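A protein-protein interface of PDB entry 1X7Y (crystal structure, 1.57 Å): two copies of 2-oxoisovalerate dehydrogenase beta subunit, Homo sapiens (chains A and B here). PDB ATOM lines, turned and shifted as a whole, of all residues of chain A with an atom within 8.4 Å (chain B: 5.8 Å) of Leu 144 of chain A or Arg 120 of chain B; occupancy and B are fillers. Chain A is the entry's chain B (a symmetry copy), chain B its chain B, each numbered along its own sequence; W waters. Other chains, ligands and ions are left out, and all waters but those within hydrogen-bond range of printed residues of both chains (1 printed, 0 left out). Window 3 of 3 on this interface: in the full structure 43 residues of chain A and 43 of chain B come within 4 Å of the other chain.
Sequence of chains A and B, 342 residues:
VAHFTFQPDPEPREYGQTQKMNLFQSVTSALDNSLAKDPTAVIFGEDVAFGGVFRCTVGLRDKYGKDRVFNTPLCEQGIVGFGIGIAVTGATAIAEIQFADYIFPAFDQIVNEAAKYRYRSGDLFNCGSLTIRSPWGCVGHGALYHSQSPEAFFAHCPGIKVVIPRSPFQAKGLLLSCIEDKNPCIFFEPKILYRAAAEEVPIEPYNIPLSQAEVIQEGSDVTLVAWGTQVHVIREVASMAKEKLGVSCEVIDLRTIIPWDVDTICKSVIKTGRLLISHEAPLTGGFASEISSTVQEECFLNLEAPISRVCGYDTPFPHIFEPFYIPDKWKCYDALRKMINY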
ATOM      1  N   ALA A 100     -41.875   5.710   2.634  1.00  0.00           N
ATOM      2  CA  ALA A 100     -41.846   4.381   1.924  1.00  0.00           C
ATOM      3  C   ALA A 100     -40.464   3.739   2.107  1.00  0.00           C
ATOM      4  O   ALA A 100     -40.386   2.506   2.070  1.00  0.00           O
ATOM      5  CB  ALA A 100     -42.151   4.550   0.409  1.00  0.00           C
ATOM      6  N   ASP A 101     -39.401   4.537   2.271  1.00  0.00           N
ATOM      7  CA  ASP A 101     -38.061   4.063   2.556  1.00  0.00           C
ATOM      8  C   ASP A 101     -38.004   3.140   3.769  1.00  0.00           C
ATOM      9  O   ASP A 101     -37.092   2.322   3.861  1.00  0.00           O
ATOM     10  CB  ASP A 101     -37.186   5.272   2.830  1.00  0.00           C
ATOM     11  CG  ASP A 101     -37.374   6.400   1.793  1.00  0.00           C
ATOM     12  OD1 ASP A 101     -38.442   7.063   1.813  1.00  0.00           O
ATOM     13  OD2 ASP A 101     -36.444   6.643   0.981  1.00  0.00           O
ATOM     14  N   TYR A 102     -38.938   3.269   4.726  1.00  0.00           N
ATOM     15  CA  TYR A 102     -38.951   2.476   5.955  1.00  0.00           C
ATOM     16  C   TYR A 102     -39.981   1.391   5.901  1.00  0.00           C
ATOM     17  O   TYR A 102     -40.355   0.839   6.904  1.00  0.00           O
ATOM     18  CB  TYR A 102     -39.206   3.400   7.174  1.00  0.00           C
ATOM     19  CG  TYR A 102     -38.224   4.568   7.286  1.00  0.00           C
ATOM     20  CD1 TYR A 102     -36.842   4.411   7.016  1.00  0.00           C
ATOM     21  CD2 TYR A 102     -38.717   5.847   7.594  1.00  0.00           C
ATOM     22  CE1 TYR A 102     -35.956   5.463   7.101  1.00  0.00           C
ATOM     23  CE2 TYR A 102     -37.810   6.957   7.672  1.00  0.00           C
ATOM     24  CZ  TYR A 102     -36.455   6.720   7.417  1.00  0.00           C
ATOM     25  OH  TYR A 102     -35.553   7.764   7.458  1.00  0.00           O
ATOM     26  N   PHE A 104     -39.298  -1.443   4.368  1.00  0.00           N
ATOM     27  CA  PHE A 104     -38.542  -2.691   4.276  1.00  0.00           C
ATOM     28  C   PHE A 104     -38.514  -3.578   5.526  1.00  0.00           C
ATOM     29  O   PHE A 104     -38.517  -4.785   5.376  1.00  0.00           O
ATOM     30  CB  PHE A 104     -37.155  -2.455   3.670  1.00  0.00           C
ATOM     31  CG  PHE A 104     -37.229  -1.816   2.290  1.00  0.00           C
ATOM     32  CD1 PHE A 104     -37.988  -2.389   1.247  1.00  0.00           C
ATOM     33  CD2 PHE A 104     -36.604  -0.599   2.088  1.00  0.00           C
ATOM     34  CE1 PHE A 104     -38.030  -1.761  -0.022  1.00  0.00           C
ATOM     35  CE2 PHE A 104     -36.693   0.072   0.844  1.00  0.00           C
ATOM     36  CZ  PHE A 104     -37.385  -0.518  -0.209  1.00  0.00           C
ATOM     37  N   HIS A 141     -34.526  17.004  -1.622  1.00  0.00           N
ATOM     38  CA  HIS A 141     -33.415  16.913  -0.696  1.00  0.00           C
ATOM     39  C   HIS A 141     -33.503  15.739   0.239  1.00  0.00           C
ATOM     40  O   HIS A 141     -32.818  15.733   1.273  1.00  0.00           O
ATOM     41  CB  HIS A 141     -33.441  18.180   0.164  1.00  0.00           C
ATOM     42  CG  HIS A 141     -34.830  18.530   0.623  1.00  0.00           C
ATOM     43  ND1 HIS A 141     -35.592  19.517   0.025  1.00  0.00           N
ATOM     44  CD2 HIS A 141     -35.623  17.967   1.568  1.00  0.00           C
ATOM     45  CE1 HIS A 141     -36.782  19.562   0.602  1.00  0.00           C
ATOM     46  NE2 HIS A 141     -36.819  18.645   1.553  1.00  0.00           N
ATOM     47  N   GLY A 142     -34.338  14.748  -0.101  1.00  0.00           N
ATOM     48  CA  GLY A 142     -34.589  13.607   0.785  1.00  0.00           C
ATOM     49  C   GLY A 142     -33.435  12.606   0.859  1.00  0.00           C
ATOM     50  O   GLY A 142     -33.439  11.753   1.746  1.00  0.00           O
ATOM     51  N   ALA A 143     -32.527  12.639  -0.122  1.00  0.00           N
ATOM     52  CA  ALA A 143     -31.376  11.730  -0.150  1.00  0.00           C
ATOM     53  C   ALA A 143     -31.823  10.268  -0.069  1.00  0.00           C
ATOM     54  O   ALA A 143     -32.826   9.887  -0.671  1.00  0.00           O
ATOM     55  CB  ALA A 143     -30.313  12.135   0.946  1.00  0.00           C
ATOM     56  N   LEU A 144     -31.052   9.425   0.622  1.00  0.00           N
ATOM     57  CA  LEU A 144     -31.177   7.960   0.409  1.00  0.00           C
ATOM     58  C   LEU A 144     -32.435   7.389   1.017  1.00  0.00           C
ATOM     59  O   LEU A 144     -32.965   6.425   0.484  1.00  0.00           O
ATOM     60  CB  LEU A 144     -29.962   7.192   0.985  1.00  0.00           C
ATOM     61  CG  LEU A 144     -28.716   7.083   0.090  1.00  0.00           C
ATOM     62  CD1 LEU A 144     -27.956   8.417   0.064  1.00  0.00           C
ATOM     63  CD2 LEU A 144     -27.837   5.949   0.708  1.00  0.00           C
ATOM     64  N   TYR A 145     -32.933   8.034   2.080  1.00  0.00           N
ATOM     65  CA  TYR A 145     -33.950   7.411   2.914  1.00  0.00           C
ATOM     66  C   TYR A 145     -35.222   8.234   3.087  1.00  0.00           C
ATOM     67  O   TYR A 145     -36.085   7.861   3.885  1.00  0.00           O
ATOM     68  CB  TYR A 145     -33.385   6.934   4.294  1.00  0.00           C
ATOM     69  CG  TYR A 145     -32.169   6.065   4.132  1.00  0.00           C
ATOM     70  CD1 TYR A 145     -32.308   4.754   3.662  1.00  0.00           C
ATOM     71  CD2 TYR A 145     -30.891   6.560   4.389  1.00  0.00           C
ATOM     72  CE1 TYR A 145     -31.146   3.953   3.473  1.00  0.00           C
ATOM     73  CE2 TYR A 145     -29.713   5.750   4.215  1.00  0.00           C
ATOM     74  CZ  TYR A 145     -29.892   4.450   3.773  1.00  0.00           C
ATOM     75  OH  TYR A 145     -28.781   3.632   3.539  1.00  0.00           O
ATOM     76  N   HIS A 146     -35.320   9.341   2.355  1.00  0.00           N
ATOM     77  CA  HIS A 146     -36.549  10.116   2.309  1.00  0.00           C
ATOM     78  C   HIS A 146     -37.140  10.253   0.890  1.00  0.00           C
ATOM     79  O   HIS A 146     -38.108  11.014   0.688  1.00  0.00           O
ATOM     80  CB  HIS A 146     -36.289  11.511   2.885  1.00  0.00           C
ATOM     81  CG  HIS A 146     -36.404  11.592   4.379  1.00  0.00           C
ATOM     82  ND1 HIS A 146     -36.524  12.809   5.010  1.00  0.00           N
ATOM     83  CD2 HIS A 146     -36.413  10.653   5.367  1.00  0.00           C
ATOM     84  CE1 HIS A 146     -36.611  12.621   6.314  1.00  0.00           C
ATOM     85  NE2 HIS A 146     -36.533  11.328   6.558  1.00  0.00           N
ATOM     86  N   SER A 147     -36.569   9.503  -0.048  1.00  0.00           N
ATOM     87  CA  SER A 147     -36.805   9.711  -1.472  1.00  0.00           C
ATOM     88  C   SER A 147     -37.293   8.495  -2.223  1.00  0.00           C
ATOM     89  O   SER A 147     -37.614   8.626  -3.389  1.00  0.00           O
ATOM     90  CB  SER A 147     -35.502  10.119  -2.188  1.00  0.00           C
ATOM     91  OG  SER A 147     -34.926  11.251  -1.549  1.00  0.00           O
ATOM     92  N   GLN A 148     -37.222   7.307  -1.613  1.00  0.00           N
ATOM     93  CA  GLN A 148     -37.304   6.079  -2.443  1.00  0.00           C
ATOM     94  C   GLN A 148     -38.683   5.827  -3.065  1.00  0.00           C
ATOM     95  O   GLN A 148     -39.742   6.293  -2.546  1.00  0.00           O
ATOM     96  CB  GLN A 148     -36.922   4.828  -1.633  1.00  0.00           C
ATOM     97  CG  GLN A 148     -35.402   4.794  -1.377  1.00  0.00           C
ATOM     98  CD  GLN A 148     -34.994   3.554  -0.611  1.00  0.00           C
ATOM     99  OE1 GLN A 148     -35.352   2.438  -1.026  1.00  0.00           O
ATOM    100  NE2 GLN A 148     -34.275   3.726   0.505  1.00  0.00           N
ATOM    101  N   SER A 149     -38.651   5.073  -4.162  1.00  0.00           N
ATOM    102  CA  SER A 149     -39.839   4.643  -4.893  1.00  0.00           C
ATOM    103  C   SER A 149     -39.791   3.101  -4.926  1.00  0.00           C
ATOM    104  O   SER A 149     -39.144   2.534  -5.851  1.00  0.00           O
ATOM    105  CB  SER A 149     -39.733   5.114  -6.364  1.00  0.00           C
ATOM    106  OG  SER A 149     -39.973   6.502  -6.453  1.00  0.00           O
ATOM    107  N   THR A 315     -28.195   3.663  -8.764  1.00  0.00           N
ATOM    108  CA  THR A 315     -27.453   4.110  -7.560  1.00  0.00           C
ATOM    109  C   THR A 315     -28.480   4.280  -6.436  1.00  0.00           C
ATOM    110  O   THR A 315     -29.696   4.358  -6.720  1.00  0.00           O
ATOM    111  CB  THR A 315     -26.693   5.496  -7.817  1.00  0.00           C
ATOM    112  OG1 THR A 315     -27.689   6.539  -7.962  1.00  0.00           O
ATOM    113  CG2 THR A 315     -25.916   5.489  -9.156  1.00  0.00           C
ATOM    114  N   PRO A 316     -28.006   4.427  -5.201  1.00  0.00           N
ATOM    115  CA  PRO A 316     -28.913   4.929  -4.140  1.00  0.00           C
ATOM    116  C   PRO A 316     -29.254   6.395  -4.480  1.00  0.00           C
ATOM    117  O   PRO A 316     -28.597   7.029  -5.338  1.00  0.00           O
ATOM    118  CB  PRO A 316     -28.048   4.846  -2.882  1.00  0.00           C
ATOM    119  CG  PRO A 316     -26.979   3.790  -3.245  1.00  0.00           C
ATOM    120  CD  PRO A 316     -26.635   4.139  -4.694  1.00  0.00           C
ATOM    121  N   PHE A 317     -30.279   6.912  -3.818  1.00  0.00           N
ATOM    122  CA  PHE A 317     -30.799   8.220  -4.164  1.00  0.00           C
ATOM    123  C   PHE A 317     -29.976   9.318  -3.495  1.00  0.00           C
ATOM    124  O   PHE A 317     -29.994   9.431  -2.255  1.00  0.00           O
ATOM    125  CB  PHE A 317     -32.302   8.300  -3.785  1.00  0.00           C
ATOM    126  CG  PHE A 317     -33.001   9.416  -4.484  1.00  0.00           C
ATOM    127  CD1 PHE A 317     -32.701  10.723  -4.152  1.00  0.00           C
ATOM    128  CD2 PHE A 317     -33.880   9.132  -5.542  1.00  0.00           C
ATOM    129  CE1 PHE A 317     -33.287  11.775  -4.881  1.00  0.00           C
ATOM    130  CE2 PHE A 317     -34.503  10.188  -6.278  1.00  0.00           C
ATOM    131  CZ  PHE A 317     -34.220  11.507  -5.911  1.00  0.00           C
ATOM    132  N   PRO A 318     -29.268  10.144  -4.243  1.00  0.00           N
ATOM    133  CA  PRO A 318     -28.312  11.056  -3.581  1.00  0.00           C
ATOM    134  C   PRO A 318     -28.937  12.352  -3.029  1.00  0.00           C
ATOM    135  O   PRO A 318     -29.960  12.868  -3.531  1.00  0.00           O
ATOM    136  CB  PRO A 318     -27.331  11.396  -4.720  1.00  0.00           C
ATOM    137  CG  PRO A 318     -28.249  11.449  -5.976  1.00  0.00           C
ATOM    138  CD  PRO A 318     -29.233  10.257  -5.721  1.00  0.00           C
ATOM    139  N   HIS A 319     -28.269  12.905  -2.021  1.00  0.00           N
ATOM    140  CA  HIS A 319     -28.624  14.235  -1.492  1.00  0.00           C
ATOM    141  C   HIS A 319     -28.272  15.378  -2.488  1.00  0.00           C
ATOM    142  O   HIS A 319     -29.160  15.903  -3.184  1.00  0.00           O
ATOM    143  CB  HIS A 319     -27.899  14.481  -0.149  1.00  0.00           C
ATOM    144  CG  HIS A 319     -28.186  15.828   0.449  1.00  0.00           C
ATOM    145  ND1 HIS A 319     -27.217  16.618   1.041  1.00  0.00           N
ATOM    146  CD2 HIS A 319     -29.360  16.494   0.581  1.00  0.00           C
ATOM    147  CE1 HIS A 319     -27.777  17.745   1.466  1.00  0.00           C
ATOM    148  NE2 HIS A 319     -29.075  17.688   1.203  1.00  0.00           N
ATOM    149  N   ILE A 320     -27.001  15.801  -2.516  1.00  0.00           N
ATOM    150  CA  ILE A 320     -26.639  17.031  -3.265  1.00  0.00           C
ATOM    151  C   ILE A 320     -26.835  16.864  -4.776  1.00  0.00           C
ATOM    152  O   ILE A 320     -27.019  17.868  -5.501  1.00  0.00           O
ATOM    153  CB  ILE A 320     -25.215  17.533  -2.846  1.00  0.00           C
ATOM    154  CG1 ILE A 320     -25.111  19.059  -3.011  1.00  0.00           C
ATOM    155  CG2 ILE A 320     -24.064  16.787  -3.564  1.00  0.00           C
ATOM    156  CD1 ILE A 320     -26.055  19.766  -1.991  1.00  0.00           C
ATOM    157  N   GLU A 322     -29.271  15.324  -6.408  1.00  0.00           N
ATOM    158  CA  GLU A 322     -30.625  15.020  -6.888  1.00  0.00           C
ATOM    159  C   GLU A 322     -30.949  15.657  -8.254  1.00  0.00           C
ATOM    160  O   GLU A 322     -31.531  14.940  -9.090  1.00  0.00           O
ATOM    161  CB  GLU A 322     -31.705  15.369  -5.833  1.00  0.00           C
ATOM    162  CG  GLU A 322     -33.125  15.160  -6.356  1.00  0.00           C
ATOM    163  CD  GLU A 322     -34.195  15.089  -5.290  1.00  0.00           C
ATOM    164  OE1 GLU A 322     -33.867  14.930  -4.096  1.00  0.00           O
ATOM    165  OE2 GLU A 322     -35.386  15.188  -5.643  1.00  0.00           O
ATOM    166  N   ASN B 112     -31.482  -1.473   2.600  1.00  0.00           N
ATOM    167  CA  ASN B 112     -31.199  -0.125   3.132  1.00  0.00           C
ATOM    168  C   ASN B 112     -29.822  -0.014   3.719  1.00  0.00           C
ATOM    169  O   ASN B 112     -29.210   1.072   3.653  1.00  0.00           O
ATOM    170  CB  ASN B 112     -32.258   0.308   4.158  1.00  0.00           C
ATOM    171  CG  ASN B 112     -33.377   1.094   3.546  1.00  0.00           C
ATOM    172  OD1 ASN B 112     -33.265   1.581   2.415  1.00  0.00           O
ATOM    173  ND2 ASN B 112     -34.490   1.197   4.304  1.00  0.00           N
ATOM    174  N   GLU B 113     -29.261  -1.132   4.190  1.00  0.00           N
ATOM    175  CA  GLU B 113     -27.941  -1.041   4.861  1.00  0.00           C
ATOM    176  C   GLU B 113     -26.826  -1.636   4.010  1.00  0.00           C
ATOM    177  O   GLU B 113     -25.990  -0.909   3.542  1.00  0.00           O
ATOM    178  CB  GLU B 113     -28.014  -1.696   6.255  1.00  0.00           C
ATOM    179  CG  GLU B 113     -28.940  -0.924   7.208  1.00  0.00           C
ATOM    180  CD  GLU B 113     -28.372   0.387   7.665  1.00  0.00           C
ATOM    181  OE1 GLU B 113     -27.267   0.405   8.194  1.00  0.00           O
ATOM    182  OE2 GLU B 113     -29.057   1.431   7.454  1.00  0.00           O
ATOM    183  N   LYS B 116     -26.067  -0.097   0.493  1.00  0.00           N
ATOM    184  CA  LYS B 116     -25.805   1.323   0.508  1.00  0.00           C
ATOM    185  C   LYS B 116     -24.623   1.757   1.364  1.00  0.00           C
ATOM    186  O   LYS B 116     -24.248   2.969   1.368  1.00  0.00           O
ATOM    187  CB  LYS B 116     -27.105   2.062   0.892  1.00  0.00           C
ATOM    188  CG  LYS B 116     -28.249   1.858  -0.135  1.00  0.00           C
ATOM    189  CD  LYS B 116     -29.541   2.355   0.491  1.00  0.00           C
ATOM    190  CE  LYS B 116     -30.658   2.329  -0.576  1.00  0.00           C
ATOM    191  NZ  LYS B 116     -30.800   0.963  -1.248  1.00  0.00           N
ATOM    192  N   TYR B 117     -23.994   0.812   2.047  1.00  0.00           N
ATOM    193  CA  TYR B 117     -23.004   1.111   3.092  1.00  0.00           C
ATOM    194  C   TYR B 117     -21.804   1.892   2.519  1.00  0.00           C
ATOM    195  O   TYR B 117     -21.364   2.889   3.088  1.00  0.00           O
ATOM    196  CB  TYR B 117     -22.498  -0.252   3.701  1.00  0.00           C
ATOM    197  CG  TYR B 117     -22.431  -0.172   5.198  1.00  0.00           C
ATOM    198  CD1 TYR B 117     -23.542  -0.606   5.921  1.00  0.00           C
ATOM    199  CD2 TYR B 117     -21.298   0.302   5.912  1.00  0.00           C
ATOM    200  CE1 TYR B 117     -23.571  -0.553   7.314  1.00  0.00           C
ATOM    201  CE2 TYR B 117     -21.307   0.332   7.309  1.00  0.00           C
ATOM    202  CZ  TYR B 117     -22.438  -0.114   7.992  1.00  0.00           C
ATOM    203  OH  TYR B 117     -22.488   0.001   9.371  1.00  0.00           O
ATOM    204  N   ARG B 118     -21.276   1.440   1.397  1.00  0.00           N
ATOM    205  CA  ARG B 118     -20.100   2.048   0.824  1.00  0.00           C
ATOM    206  C   ARG B 118     -20.435   3.436   0.199  1.00  0.00           C
ATOM    207  O   ARG B 118     -19.773   4.459   0.470  1.00  0.00           O
ATOM    208  CB  ARG B 118     -19.514   1.133  -0.258  1.00  0.00           C
ATOM    209  CG  ARG B 118     -18.134   1.663  -0.682  1.00  0.00           C
ATOM    210  CD  ARG B 118     -17.430   0.848  -1.865  1.00  0.00           C
ATOM    211  NE  ARG B 118     -17.213  -0.568  -1.481  1.00  0.00           N
ATOM    212  CZ  ARG B 118     -16.126  -1.043  -0.869  1.00  0.00           C
ATOM    213  NH1 ARG B 118     -15.138  -0.252  -0.446  1.00  0.00           N
ATOM    214  NH2 ARG B 118     -16.038  -2.353  -0.647  1.00  0.00           N
ATOM    215  N   TYR B 119     -21.513   3.472  -0.579  1.00  0.00           N
ATOM    216  CA  TYR B 119     -21.903   4.706  -1.239  1.00  0.00           C
ATOM    217  C   TYR B 119     -22.155   5.828  -0.209  1.00  0.00           C
ATOM    218  O   TYR B 119     -21.643   6.942  -0.340  1.00  0.00           O
ATOM    219  CB  TYR B 119     -23.217   4.436  -2.002  1.00  0.00           C
ATOM    220  CG  TYR B 119     -23.646   5.593  -2.872  1.00  0.00           C
ATOM    221  CD1 TYR B 119     -23.047   5.827  -4.115  1.00  0.00           C
ATOM    222  CD2 TYR B 119     -24.738   6.382  -2.474  1.00  0.00           C
ATOM    223  CE1 TYR B 119     -23.506   6.856  -4.936  1.00  0.00           C
ATOM    224  CE2 TYR B 119     -25.208   7.436  -3.297  1.00  0.00           C
ATOM    225  CZ  TYR B 119     -24.609   7.616  -4.527  1.00  0.00           C
ATOM    226  OH  TYR B 119     -25.030   8.627  -5.363  1.00  0.00           O
ATOM    227  N   ARG B 120     -23.000   5.533   0.783  1.00  0.00           N
ATOM    228  CA  ARG B 120     -23.469   6.579   1.674  1.00  0.00           C
ATOM    229  C   ARG B 120     -22.366   7.114   2.594  1.00  0.00           C
ATOM    230  O   ARG B 120     -22.508   8.172   3.217  1.00  0.00           O
ATOM    231  CB  ARG B 120     -24.673   6.085   2.508  1.00  0.00           C
ATOM    232  CG  ARG B 120     -24.260   5.189   3.712  1.00  0.00           C
ATOM    233  CD  ARG B 120     -25.462   4.487   4.243  1.00  0.00           C
ATOM    234  NE  ARG B 120     -25.012   3.717   5.372  1.00  0.00           N
ATOM    235  CZ  ARG B 120     -25.813   2.880   6.054  1.00  0.00           C
ATOM    236  NH1 ARG B 120     -27.070   2.645   5.623  1.00  0.00           N
ATOM    237  NH2 ARG B 120     -25.342   2.263   7.152  1.00  0.00           N
ATOM    238  N   SER B 121     -21.283   6.372   2.733  1.00  0.00           N
ATOM    239  CA  SER B 121     -20.177   6.811   3.570  1.00  0.00           C
ATOM    240  C   SER B 121     -19.054   7.477   2.758  1.00  0.00           C
ATOM    241  O   SER B 121     -18.001   7.858   3.351  1.00  0.00           O
ATOM    242  CB  SER B 121     -19.604   5.634   4.434  1.00  0.00           C
ATOM    243  OG  SER B 121     -18.944   4.714   3.538  1.00  0.00           O
ATOM    244  N   GLY B 122     -19.205   7.620   1.431  1.00  0.00           N
ATOM    245  CA  GLY B 122     -18.099   8.074   0.581  1.00  0.00           C
ATOM    246  C   GLY B 122     -16.906   7.142   0.621  1.00  0.00           C
ATOM    247  O   GLY B 122     -15.773   7.571   0.487  1.00  0.00           O
ATOM    248  N   ASP B 123     -17.173   5.851   0.842  1.00  0.00           N
ATOM    249  CA  ASP B 123     -16.137   4.840   0.998  1.00  0.00           C
ATOM    250  C   ASP B 123     -15.327   4.990   2.274  1.00  0.00           C
ATOM    251  O   ASP B 123     -14.249   4.410   2.361  1.00  0.00           O
ATOM    252  CB  ASP B 123     -15.210   4.773  -0.256  1.00  0.00           C
ATOM    253  CG  ASP B 123     -14.398   3.487  -0.317  1.00  0.00           C
ATOM    254  OD1 ASP B 123     -14.957   2.449   0.010  1.00  0.00           O
ATOM    255  OD2 ASP B 123     -13.190   3.488  -0.677  1.00  0.00           O
HETATM  256  O   HOH W   1     -33.415   1.009  -2.468  1.00  0.00           O
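ND2 of Asn 112 of chain B sits at hydrogen-bond distance from O of Asp 101 of chain A (2.9 Å).
The side-chain hydroxyl (OH) of Tyr 145 of chain A is in hydrogen-bond range of the backbone carbonyl oxygen (O) of Asn 112 of chain B, at 2.6 Å.
The side-chain amide nitrogen (NE2) of Gln 148 of chain A is in hydrogen-bond range of the side-chain amide oxygen (OD1) of Asn 112 of chain B.
The guanidinium group (NH1) of Arg 120 of chain B lies within hydrogen-bond range of the side-chain hydroxyl (OH) of Tyr 145 of chain A, 2.9 Å away.
The backbone carbonyl oxygen (O) of Asn 112 of chain B lies within hydrogen-bond range of the guanidinium group (NH1) of Arg 120 of chain B.
The side-chain carboxylate of Glu 113 of chain B is in salt-bridge range of the guanidinium group of Arg 120 of chain B (2.9 Å).
OD2 of Asp 101 of chain A lies within hydrogen-bond range of N of His 146 of chain A (3.2 Å).
OD2 of Asp 101 of chain A lies within hydrogen-bond range of N of Gln 148 of chain A (2.8 Å).
The backbone carbonyl oxygen (O) of Leu 144 of chain A lies within hydrogen-bond range of the side-chain amide nitrogen (NE2) of Gln 148 of chain A, 3.0 Å away.
O of Phe 317 of chain A sits at hydrogen-bond distance from N of Leu 144 of chain A, at 3.1 Å.
Phe 104 of chain A touches Asn 112 of chain B (CD2 to ND2, 3.6 Å).
Leu 144 of chain A touches Lys 116 of chain B.
Leu 144 of chain A touches Arg 120 of chain B (CD2 to CB, 3.6 Å).
Lys 116 of chain B touches Tyr 145 of chain A.
Lys 116 of chain B touches Pro 316 of chain A.
Pro 316 of chain A touches Tyr 119 of chain B (CG to CD2, 3.5 Å).
Pro 318 of chain A touches Tyr 119 of chain B.
Of chain B, only Lys 116 and Arg 120 come within 4 Å of Leu 144 of chain A.
Of the printed residues of chain A, Arg 120 of chain B touches Leu 144 and Tyr 145.
Of the printed residues of chain B, Gln 148 of chain A touches Asn 112 (3.0 Å).
Of the printed residues of chain B, Pro 316 of chain A touches Lys 116 and Tyr 119.
Phe 317 of chain A touches none of the printed residues of chain B.
Asp 123 of chain B touches none of the printed residues of chain A.
The nearest residue of chain B that does not touch Leu 144 of chain A is Tyr 119 of chain B (4.5 Å).
The nearest residue of chain A that does not touch Arg 120 of chain B is Pro 316 of chain A (5.9 Å).
The nearest printed residue of chain B that does not touch Asp 101 of chain A is Lys 116 of chain B (7.4 Å).
Printed residues of chain A that touch a printed residue of chain B: Asp 101, Phe 104, Leu 144, Tyr 145, Gln 148, Pro 316 and Pro 318.
Hydrophobic or aromatic side chains of chain A that line the printed part of chain B: Phe 104, Leu 144, Tyr 145, Pro 316 and Pro 318.
Hydrophobic or aromatic side chains of chain B that line the printed part of chain A: Tyr 119.
Among the printed residues, 11 pairs touch across the chains.
No position is printed for both chains.
Water W1 lies within hydrogen-bond range of OE1 of Gln 148 of chain A (2.8 Å) and NZ of Lys 116 of chain B (2.9 Å).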
